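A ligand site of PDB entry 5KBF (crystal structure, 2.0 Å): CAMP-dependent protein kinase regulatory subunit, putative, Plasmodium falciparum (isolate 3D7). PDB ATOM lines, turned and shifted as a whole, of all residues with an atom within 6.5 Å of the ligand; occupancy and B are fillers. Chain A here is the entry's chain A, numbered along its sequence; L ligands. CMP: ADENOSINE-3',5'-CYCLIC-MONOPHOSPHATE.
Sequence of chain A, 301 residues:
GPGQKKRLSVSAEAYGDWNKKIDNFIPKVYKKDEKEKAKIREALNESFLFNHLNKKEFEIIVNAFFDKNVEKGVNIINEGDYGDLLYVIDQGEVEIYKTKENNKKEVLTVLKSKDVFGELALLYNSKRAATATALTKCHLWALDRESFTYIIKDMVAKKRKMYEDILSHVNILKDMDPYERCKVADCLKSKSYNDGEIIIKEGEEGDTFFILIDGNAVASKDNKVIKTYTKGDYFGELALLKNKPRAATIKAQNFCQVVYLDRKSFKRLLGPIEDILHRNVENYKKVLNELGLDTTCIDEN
The side-chain carboxylate of Glu 119 is in hydrogen-bond range of an oxygen (O2') of the ligand (2.7 Å).
O1P of the ligand lies within hydrogen-bond range of N of Ala 129.
The backbone NH of Gly 118 sits at hydrogen-bond distance from an oxygen (O2') of the ligand, at 2.8 Å.
The guanidinium group (NH1) of Arg 128 lies within salt-bridge range of an oxygen (O2P) of the ligand, 2.9 Å away.
The backbone NH (N) of Ala 121 lies within hydrogen-bond range of an oxygen (O2P) of the ligand (3.2 Å).
An oxygen (O2') of the ligand sits at hydrogen-bond distance from the side-chain hydroxyl (OH) of Tyr 179, 3.3 Å away.
The side-chain carboxylate (OD1) of Asp 177 sits at hydrogen-bond distance from a nitrogen (N6) of the ligand, at 3.3 Å.
OE2 of Glu 119 is in hydrogen-bond range of OH of Tyr 179 (2.7 Å).
NZ of Lys 98 is in hydrogen-bond range of O of Ala 129 (3.0 Å).
The backbone carbonyl oxygen (O) of Gly 118 sits at hydrogen-bond distance from the guanidinium group (NH1) of Arg 128 (2.9 Å).
The backbone carbonyl oxygen (O) of Leu 85 lies within hydrogen-bond range of the guanidinium group (NH2) of Arg 128.
N of Tyr 179 sits at hydrogen-bond distance from OD2 of Asp 177, at 2.6 Å.
The backbone carbonyl oxygen (O) of Ile 96 sits at hydrogen-bond distance from the backbone NH (N) of Leu 108 (2.8 Å).
N of Ile 96 is in hydrogen-bond range of O of Thr 109 (2.8 Å).
CG2 of Ile 96 touches O4' of the ligand, at 3.5 Å.
Leu 108 touches the ligand (CD1 to C6, 3.5 Å).
Thr 109 touches the ligand.
CA of Phe 117 touches O2' of the ligand (3.3 Å).
Leu 120 touches the ligand.
O of Ala 130 touches C5' of the ligand, at 3.7 Å.
Of the 26 residues printed, 13 come within 4 Å of the ligand.
Along chain A the residues within 4 Å of the ligand span positions 96 to 179.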
ATOM      1  N   ILE A  77      -0.510  -2.106  -4.793  1.00  0.00           N
ATOM      2  CA  ILE A  77      -1.898  -1.809  -4.429  1.00  0.00           C
ATOM      3  C   ILE A  77      -2.752  -2.974  -4.893  1.00  0.00           C
ATOM      4  O   ILE A  77      -2.561  -3.453  -6.013  1.00  0.00           O
ATOM      5  CB  ILE A  77      -2.415  -0.516  -5.109  1.00  0.00           C
ATOM      6  CG1 ILE A  77      -1.853   0.726  -4.426  1.00  0.00           C
ATOM      7  CG2 ILE A  77      -3.942  -0.481  -5.133  1.00  0.00           C
ATOM      8  CD1 ILE A  77      -2.048   0.689  -2.929  1.00  0.00           C
ATOM      9  N   GLY A  83      -7.404   2.610   1.223  1.00  0.00           N
ATOM     10  CA  GLY A  83      -6.322   3.417   0.672  1.00  0.00           C
ATOM     11  C   GLY A  83      -5.759   4.477   1.598  1.00  0.00           C
ATOM     12  O   GLY A  83      -6.485   5.352   2.080  1.00  0.00           O
ATOM     13  N   LEU A  85      -2.133   5.758   1.056  1.00  0.00           N
ATOM     14  CA  LEU A  85      -1.005   6.448   0.431  1.00  0.00           C
ATOM     15  C   LEU A  85      -1.305   6.718  -1.059  1.00  0.00           C
ATOM     16  O   LEU A  85      -2.034   5.965  -1.693  1.00  0.00           O
ATOM     17  CB  LEU A  85       0.265   5.607   0.547  1.00  0.00           C
ATOM     18  CG  LEU A  85       0.775   5.175   1.948  1.00  0.00           C
ATOM     19  CD1 LEU A  85       1.871   4.099   1.869  1.00  0.00           C
ATOM     20  CD2 LEU A  85       1.269   6.383   2.703  1.00  0.00           C
ATOM     21  N   ILE A  96      -1.368  -1.282 -14.212  1.00  0.00           N
ATOM     22  CA  ILE A  96      -2.632  -1.093 -13.528  1.00  0.00           C
ATOM     23  C   ILE A  96      -3.662  -1.956 -14.224  1.00  0.00           C
ATOM     24  O   ILE A  96      -3.810  -1.850 -15.437  1.00  0.00           O
ATOM     25  CB  ILE A  96      -3.108   0.379 -13.573  1.00  0.00           C
ATOM     26  CG1 ILE A  96      -2.021   1.324 -13.064  1.00  0.00           C
ATOM     27  CG2 ILE A  96      -4.434   0.521 -12.818  1.00  0.00           C
ATOM     28  CD1 ILE A  96      -1.829   1.293 -11.558  1.00  0.00           C
ATOM     29  N   LYS A  98      -7.595  -4.425 -13.853  1.00  0.00           N
ATOM     30  CA  LYS A  98      -8.789  -4.904 -13.179  1.00  0.00           C
ATOM     31  C   LYS A  98      -8.933  -6.383 -13.479  1.00  0.00           C
ATOM     32  O   LYS A  98      -8.555  -6.832 -14.564  1.00  0.00           O
ATOM     33  CB  LYS A  98     -10.013  -4.116 -13.643  1.00  0.00           C
ATOM     34  CG  LYS A  98     -10.792  -3.464 -12.519  1.00  0.00           C
ATOM     35  CD  LYS A  98     -11.548  -2.235 -12.990  1.00  0.00           C
ATOM     36  CE  LYS A  98     -12.456  -1.720 -11.885  1.00  0.00           C
ATOM     37  NZ  LYS A  98     -12.505  -0.239 -11.838  1.00  0.00           N
ATOM     38  N   LEU A 108      -5.629  -1.667 -17.530  1.00  0.00           N
ATOM     39  CA  LEU A 108      -6.080  -0.301 -17.757  1.00  0.00           C
ATOM     40  C   LEU A 108      -4.932   0.513 -18.357  1.00  0.00           C
ATOM     41  O   LEU A 108      -5.119   1.204 -19.354  1.00  0.00           O
ATOM     42  CB  LEU A 108      -6.593   0.329 -16.459  1.00  0.00           C
ATOM     43  CG  LEU A 108      -7.742  -0.424 -15.802  1.00  0.00           C
ATOM     44  CD1 LEU A 108      -8.222   0.226 -14.524  1.00  0.00           C
ATOM     45  CD2 LEU A 108      -8.889  -0.567 -16.771  1.00  0.00           C
ATOM     46  N   THR A 109      -3.743   0.390 -17.768  1.00  0.00           N
ATOM     47  CA  THR A 109      -2.608   1.160 -18.268  1.00  0.00           C
ATOM     48  C   THR A 109      -1.258   0.707 -17.720  1.00  0.00           C
ATOM     49  O   THR A 109      -1.177  -0.043 -16.744  1.00  0.00           O
ATOM     50  CB  THR A 109      -2.806   2.657 -17.948  1.00  0.00           C
ATOM     51  OG1 THR A 109      -1.682   3.411 -18.433  1.00  0.00           O
ATOM     52  CG2 THR A 109      -2.960   2.870 -16.452  1.00  0.00           C
ATOM     53  N   LEU A 111       2.250   2.367 -16.232  1.00  0.00           N
ATOM     54  CA  LEU A 111       2.792   3.630 -15.721  1.00  0.00           C
ATOM     55  C   LEU A 111       4.305   3.556 -15.566  1.00  0.00           C
ATOM     56  O   LEU A 111       4.860   2.483 -15.297  1.00  0.00           O
ATOM     57  CB  LEU A 111       2.135   3.981 -14.373  1.00  0.00           C
ATOM     58  CG  LEU A 111       0.615   4.175 -14.432  1.00  0.00           C
ATOM     59  CD1 LEU A 111       0.046   4.469 -13.039  1.00  0.00           C
ATOM     60  CD2 LEU A 111       0.218   5.285 -15.435  1.00  0.00           C
ATOM     61  N   VAL A 116       1.809   9.196 -11.488  1.00  0.00           N
ATOM     62  CA  VAL A 116       1.156   9.227 -10.185  1.00  0.00           C
ATOM     63  C   VAL A 116       0.067   8.165 -10.157  1.00  0.00           C
ATOM     64  O   VAL A 116      -0.670   8.018 -11.142  1.00  0.00           O
ATOM     65  CB  VAL A 116       0.513  10.614  -9.903  1.00  0.00           C
ATOM     66  CG1 VAL A 116      -0.103  10.661  -8.497  1.00  0.00           C
ATOM     67  CG2 VAL A 116       1.528  11.722 -10.093  1.00  0.00           C
ATOM     68  N   PHE A 117      -0.074   7.439  -9.056  1.00  0.00           N
ATOM     69  CA  PHE A 117      -1.237   6.567  -8.934  1.00  0.00           C
ATOM     70  C   PHE A 117      -1.638   6.399  -7.478  1.00  0.00           C
ATOM     71  O   PHE A 117      -0.828   6.640  -6.571  1.00  0.00           O
ATOM     72  CB  PHE A 117      -0.978   5.210  -9.600  1.00  0.00           C
ATOM     73  CG  PHE A 117       0.115   4.389  -8.958  1.00  0.00           C
ATOM     74  CD1 PHE A 117      -0.189   3.384  -8.041  1.00  0.00           C
ATOM     75  CD2 PHE A 117       1.452   4.598  -9.302  1.00  0.00           C
ATOM     76  CE1 PHE A 117       0.841   2.595  -7.437  1.00  0.00           C
ATOM     77  CE2 PHE A 117       2.464   3.840  -8.728  1.00  0.00           C
ATOM     78  CZ  PHE A 117       2.164   2.838  -7.791  1.00  0.00           C
ATOM     79  N   GLY A 118      -2.883   5.980  -7.262  1.00  0.00           N
ATOM     80  CA  GLY A 118      -3.386   5.760  -5.911  1.00  0.00           C
ATOM     81  C   GLY A 118      -4.059   7.001  -5.330  1.00  0.00           C
ATOM     82  O   GLY A 118      -4.326   7.052  -4.133  1.00  0.00           O
ATOM     83  N   GLU A 119      -4.335   8.000  -6.167  1.00  0.00           N
ATOM     84  CA  GLU A 119      -4.934   9.239  -5.686  1.00  0.00           C
ATOM     85  C   GLU A 119      -6.444   9.114  -5.420  1.00  0.00           C
ATOM     86  O   GLU A 119      -7.023   9.862  -4.632  1.00  0.00           O
ATOM     87  CB  GLU A 119      -4.671  10.387  -6.688  1.00  0.00           C
ATOM     88  CG  GLU A 119      -5.567  10.398  -7.937  1.00  0.00           C
ATOM     89  CD  GLU A 119      -5.195   9.317  -8.935  1.00  0.00           C
ATOM     90  OE1 GLU A 119      -4.249   8.529  -8.672  1.00  0.00           O
ATOM     91  OE2 GLU A 119      -5.828   9.256 -10.004  1.00  0.00           O
ATOM     92  N   LEU A 120      -7.110   8.172  -6.095  1.00  0.00           N
ATOM     93  CA  LEU A 120      -8.570   8.077  -6.030  1.00  0.00           C
ATOM     94  C   LEU A 120      -9.089   7.733  -4.634  1.00  0.00           C
ATOM     95  O   LEU A 120     -10.106   8.268  -4.206  1.00  0.00           O
ATOM     96  CB  LEU A 120      -9.099   7.040  -7.029  1.00  0.00           C
ATOM     97  CG  LEU A 120      -9.002   7.354  -8.516  1.00  0.00           C
ATOM     98  CD1 LEU A 120      -9.663   6.234  -9.320  1.00  0.00           C
ATOM     99  CD2 LEU A 120      -9.649   8.704  -8.839  1.00  0.00           C
ATOM    100  N   ALA A 121      -8.390   6.833  -3.940  1.00  0.00           N
ATOM    101  CA  ALA A 121      -8.789   6.461  -2.591  1.00  0.00           C
ATOM    102  C   ALA A 121      -8.672   7.658  -1.650  1.00  0.00           C
ATOM    103  O   ALA A 121      -9.489   7.836  -0.754  1.00  0.00           O
ATOM    104  CB  ALA A 121      -7.937   5.307  -2.077  1.00  0.00           C
ATOM    105  N   LEU A 122      -7.654   8.478  -1.878  1.00  0.00           N
ATOM    106  CA  LEU A 122      -7.408   9.648  -1.038  1.00  0.00           C
ATOM    107  C   LEU A 122      -8.352  10.784  -1.415  1.00  0.00           C
ATOM    108  O   LEU A 122      -8.783  11.564  -0.573  1.00  0.00           O
ATOM    109  CB  LEU A 122      -5.956  10.108  -1.185  1.00  0.00           C
ATOM    110  CG  LEU A 122      -4.826   9.104  -0.866  1.00  0.00           C
ATOM    111  CD1 LEU A 122      -3.526   9.857  -0.639  1.00  0.00           C
ATOM    112  CD2 LEU A 122      -5.160   8.232   0.326  1.00  0.00           C
ATOM    113  N   SER A 126     -12.476   5.823  -1.140  1.00  0.00           N
ATOM    114  CA  SER A 126     -13.062   4.656  -1.783  1.00  0.00           C
ATOM    115  C   SER A 126     -12.073   3.497  -1.901  1.00  0.00           C
ATOM    116  O   SER A 126     -10.852   3.722  -1.919  1.00  0.00           O
ATOM    117  CB  SER A 126     -13.565   5.034  -3.181  1.00  0.00           C
ATOM    118  OG  SER A 126     -12.539   5.704  -3.903  1.00  0.00           O
ATOM    119  N   LYS A 127     -12.593   2.282  -1.987  1.00  0.00           N
ATOM    120  CA  LYS A 127     -11.767   1.094  -2.228  1.00  0.00           C
ATOM    121  C   LYS A 127     -10.882   1.295  -3.464  1.00  0.00           C
ATOM    122  O   LYS A 127     -11.234   2.052  -4.375  1.00  0.00           O
ATOM    123  CB  LYS A 127     -12.655  -0.145  -2.409  1.00  0.00           C
ATOM    124  N   ARG A 128      -9.718   0.660  -3.475  1.00  0.00           N
ATOM    125  CA  ARG A 128      -8.824   0.798  -4.634  1.00  0.00           C
ATOM    126  C   ARG A 128      -9.506   0.282  -5.900  1.00  0.00           C
ATOM    127  O   ARG A 128      -9.994  -0.852  -5.949  1.00  0.00           O
ATOM    128  CB  ARG A 128      -7.508   0.049  -4.383  1.00  0.00           C
ATOM    129  CG  ARG A 128      -6.737   0.554  -3.179  1.00  0.00           C
ATOM    130  CD  ARG A 128      -6.121   1.945  -3.421  1.00  0.00           C
ATOM    131  NE  ARG A 128      -4.971   2.159  -2.532  1.00  0.00           N
ATOM    132  CZ  ARG A 128      -4.263   3.278  -2.483  1.00  0.00           C
ATOM    133  NH1 ARG A 128      -4.604   4.317  -3.235  1.00  0.00           N
ATOM    134  NH2 ARG A 128      -3.228   3.366  -1.658  1.00  0.00           N
ATOM    135  N   ALA A 129      -9.540   1.117  -6.926  1.00  0.00           N
ATOM    136  CA  ALA A 129     -10.330   0.828  -8.113  1.00  0.00           C
ATOM    137  C   ALA A 129      -9.645  -0.222  -8.993  1.00  0.00           C
ATOM    138  O   ALA A 129     -10.283  -0.824  -9.848  1.00  0.00           O
ATOM    139  CB  ALA A 129     -10.569   2.105  -8.911  1.00  0.00           C
ATOM    140  N   ALA A 130      -8.352  -0.447  -8.761  1.00  0.00           N
ATOM    141  CA  ALA A 130      -7.601  -1.433  -9.519  1.00  0.00           C
ATOM    142  C   ALA A 130      -6.375  -1.966  -8.748  1.00  0.00           C
ATOM    143  O   ALA A 130      -6.064  -1.495  -7.656  1.00  0.00           O
ATOM    144  CB  ALA A 130      -7.145  -0.851 -10.838  1.00  0.00           C
ATOM    145  N   THR A 131      -5.725  -2.952  -9.336  1.00  0.00           N
ATOM    146  CA  THR A 131      -4.485  -3.482  -8.796  1.00  0.00           C
ATOM    147  C   THR A 131      -3.310  -2.850  -9.520  1.00  0.00           C
ATOM    148  O   THR A 131      -3.314  -2.678 -10.743  1.00  0.00           O
ATOM    149  CB  THR A 131      -4.424  -5.018  -8.913  1.00  0.00           C
ATOM    150  OG1 THR A 131      -5.489  -5.590  -8.159  1.00  0.00           O
ATOM    151  CG2 THR A 131      -3.072  -5.534  -8.370  1.00  0.00           C
ATOM    152  N   ALA A 132      -2.300  -2.481  -8.745  1.00  0.00           N
ATOM    153  CA  ALA A 132      -1.068  -1.955  -9.309  1.00  0.00           C
ATOM    154  C   ALA A 132       0.069  -2.945  -9.023  1.00  0.00           C
ATOM    155  O   ALA A 132       0.302  -3.301  -7.871  1.00  0.00           O
ATOM    156  CB  ALA A 132      -0.777  -0.594  -8.714  1.00  0.00           C
ATOM    157  N   ASP A 177     -12.425   7.467 -21.286  1.00  0.00           N
ATOM    158  CA  ASP A 177     -12.572   6.913 -19.952  1.00  0.00           C
ATOM    159  C   ASP A 177     -12.878   8.048 -18.965  1.00  0.00           C
ATOM    160  O   ASP A 177     -12.242   9.108 -19.017  1.00  0.00           O
ATOM    161  CB  ASP A 177     -11.277   6.169 -19.561  1.00  0.00           C
ATOM    162  CG  ASP A 177     -11.393   5.406 -18.247  1.00  0.00           C
ATOM    163  OD1 ASP A 177     -10.958   4.235 -18.208  1.00  0.00           O
ATOM    164  OD2 ASP A 177     -11.873   5.963 -17.239  1.00  0.00           O
ATOM    165  N   TYR A 179     -12.113   8.199 -15.900  1.00  0.00           N
ATOM    166  CA  TYR A 179     -10.878   8.452 -15.159  1.00  0.00           C
ATOM    167  C   TYR A 179      -9.996   9.425 -15.925  1.00  0.00           C
ATOM    168  O   TYR A 179      -9.512  10.418 -15.366  1.00  0.00           O
ATOM    169  CB  TYR A 179     -10.138   7.142 -14.904  1.00  0.00           C
ATOM    170  CG  TYR A 179      -8.826   7.327 -14.207  1.00  0.00           C
ATOM    171  CD1 TYR A 179      -8.798   7.618 -12.855  1.00  0.00           C
ATOM    172  CD2 TYR A 179      -7.629   7.239 -14.894  1.00  0.00           C
ATOM    173  CE1 TYR A 179      -7.594   7.816 -12.185  1.00  0.00           C
ATOM    174  CE2 TYR A 179      -6.400   7.420 -14.228  1.00  0.00           C
ATOM    175  CZ  TYR A 179      -6.395   7.705 -12.880  1.00  0.00           C
ATOM    176  OH  TYR A 179      -5.203   7.897 -12.206  1.00  0.00           O
ATOM    177  N   GLU A 180      -9.798   9.161 -17.200  1.00  0.00           N
ATOM    178  CA  GLU A 180      -9.019  10.078 -18.018  1.00  0.00           C
ATOM    179  C   GLU A 180      -9.665  11.467 -18.148  1.00  0.00           C
ATOM    180  O   GLU A 180      -8.961  12.476 -18.213  1.00  0.00           O
ATOM    181  CB  GLU A 180      -8.786   9.465 -19.405  1.00  0.00           C
ATOM    182  CG  GLU A 180      -7.909   8.220 -19.385  1.00  0.00           C
ATOM    183  CD  GLU A 180      -6.544   8.486 -18.749  1.00  0.00           C
ATOM    184  OE1 GLU A 180      -5.959   9.560 -19.007  1.00  0.00           O
ATOM    185  OE2 GLU A 180      -6.071   7.626 -17.973  1.00  0.00           O
ATOM    186  N   LYS A 183      -9.137  14.037 -15.291  1.00  0.00           N
ATOM    187  CA  LYS A 183      -7.833  14.681 -15.438  1.00  0.00           C
ATOM    188  C   LYS A 183      -7.910  15.954 -16.265  1.00  0.00           C
ATOM    189  O   LYS A 183      -7.117  16.877 -16.054  1.00  0.00           O
ATOM    190  CB  LYS A 183      -6.844  13.717 -16.059  1.00  0.00           C
ATOM    191  CG  LYS A 183      -6.502  12.533 -15.160  1.00  0.00           C
ATOM    192  CD  LYS A 183      -5.486  11.645 -15.856  1.00  0.00           C
ATOM    193  CE  LYS A 183      -4.918  10.610 -14.901  1.00  0.00           C
ATOM    194  NZ  LYS A 183      -3.630  10.086 -15.417  1.00  0.00           N
HETATM  195  P   CMP L   1      -6.803   3.955  -6.686  1.00  0.00           P
HETATM  196  O1P CMP L   1      -8.200   3.521  -7.103  1.00  0.00           O
HETATM  197  O2P CMP L   1      -6.644   4.555  -5.342  1.00  0.00           O
HETATM  198  O5' CMP L   1      -5.981   2.625  -6.904  1.00  0.00           O
HETATM  199  C5' CMP L   1      -5.757   2.109  -8.214  1.00  0.00           C
HETATM  200  C4' CMP L   1      -5.220   3.247  -9.024  1.00  0.00           C
HETATM  201  O4' CMP L   1      -5.031   2.958 -10.408  1.00  0.00           O
HETATM  202  C3' CMP L   1      -6.140   4.428  -9.059  1.00  0.00           C
HETATM  203  O3' CMP L   1      -6.222   5.018  -7.779  1.00  0.00           O
HETATM  204  C2' CMP L   1      -5.524   5.284 -10.152  1.00  0.00           C
HETATM  205  O2' CMP L   1      -4.443   6.054  -9.636  1.00  0.00           O
HETATM  206  C1' CMP L   1      -4.948   4.200 -11.096  1.00  0.00           C
HETATM  207  N9  CMP L   1      -5.682   4.102 -12.375  1.00  0.00           N
HETATM  208  C8  CMP L   1      -5.112   4.117 -13.589  1.00  0.00           C
HETATM  209  N7  CMP L   1      -6.030   3.997 -14.564  1.00  0.00           N
HETATM  210  C5  CMP L   1      -7.220   3.882 -13.964  1.00  0.00           C
HETATM  211  C6  CMP L   1      -8.602   3.728 -14.440  1.00  0.00           C
HETATM  212  N6  CMP L   1      -8.835   3.670 -15.773  1.00  0.00           N
HETATM  213  N1  CMP L   1      -9.559   3.647 -13.498  1.00  0.00           N
HETATM  214  C2  CMP L   1      -9.307   3.699 -12.169  1.00  0.00           C
HETATM  215  N3  CMP L   1      -8.061   3.840 -11.669  1.00  0.00           N
HETATM  216  C4  CMP L   1      -7.006   3.932 -12.513  1.00  0.00           C
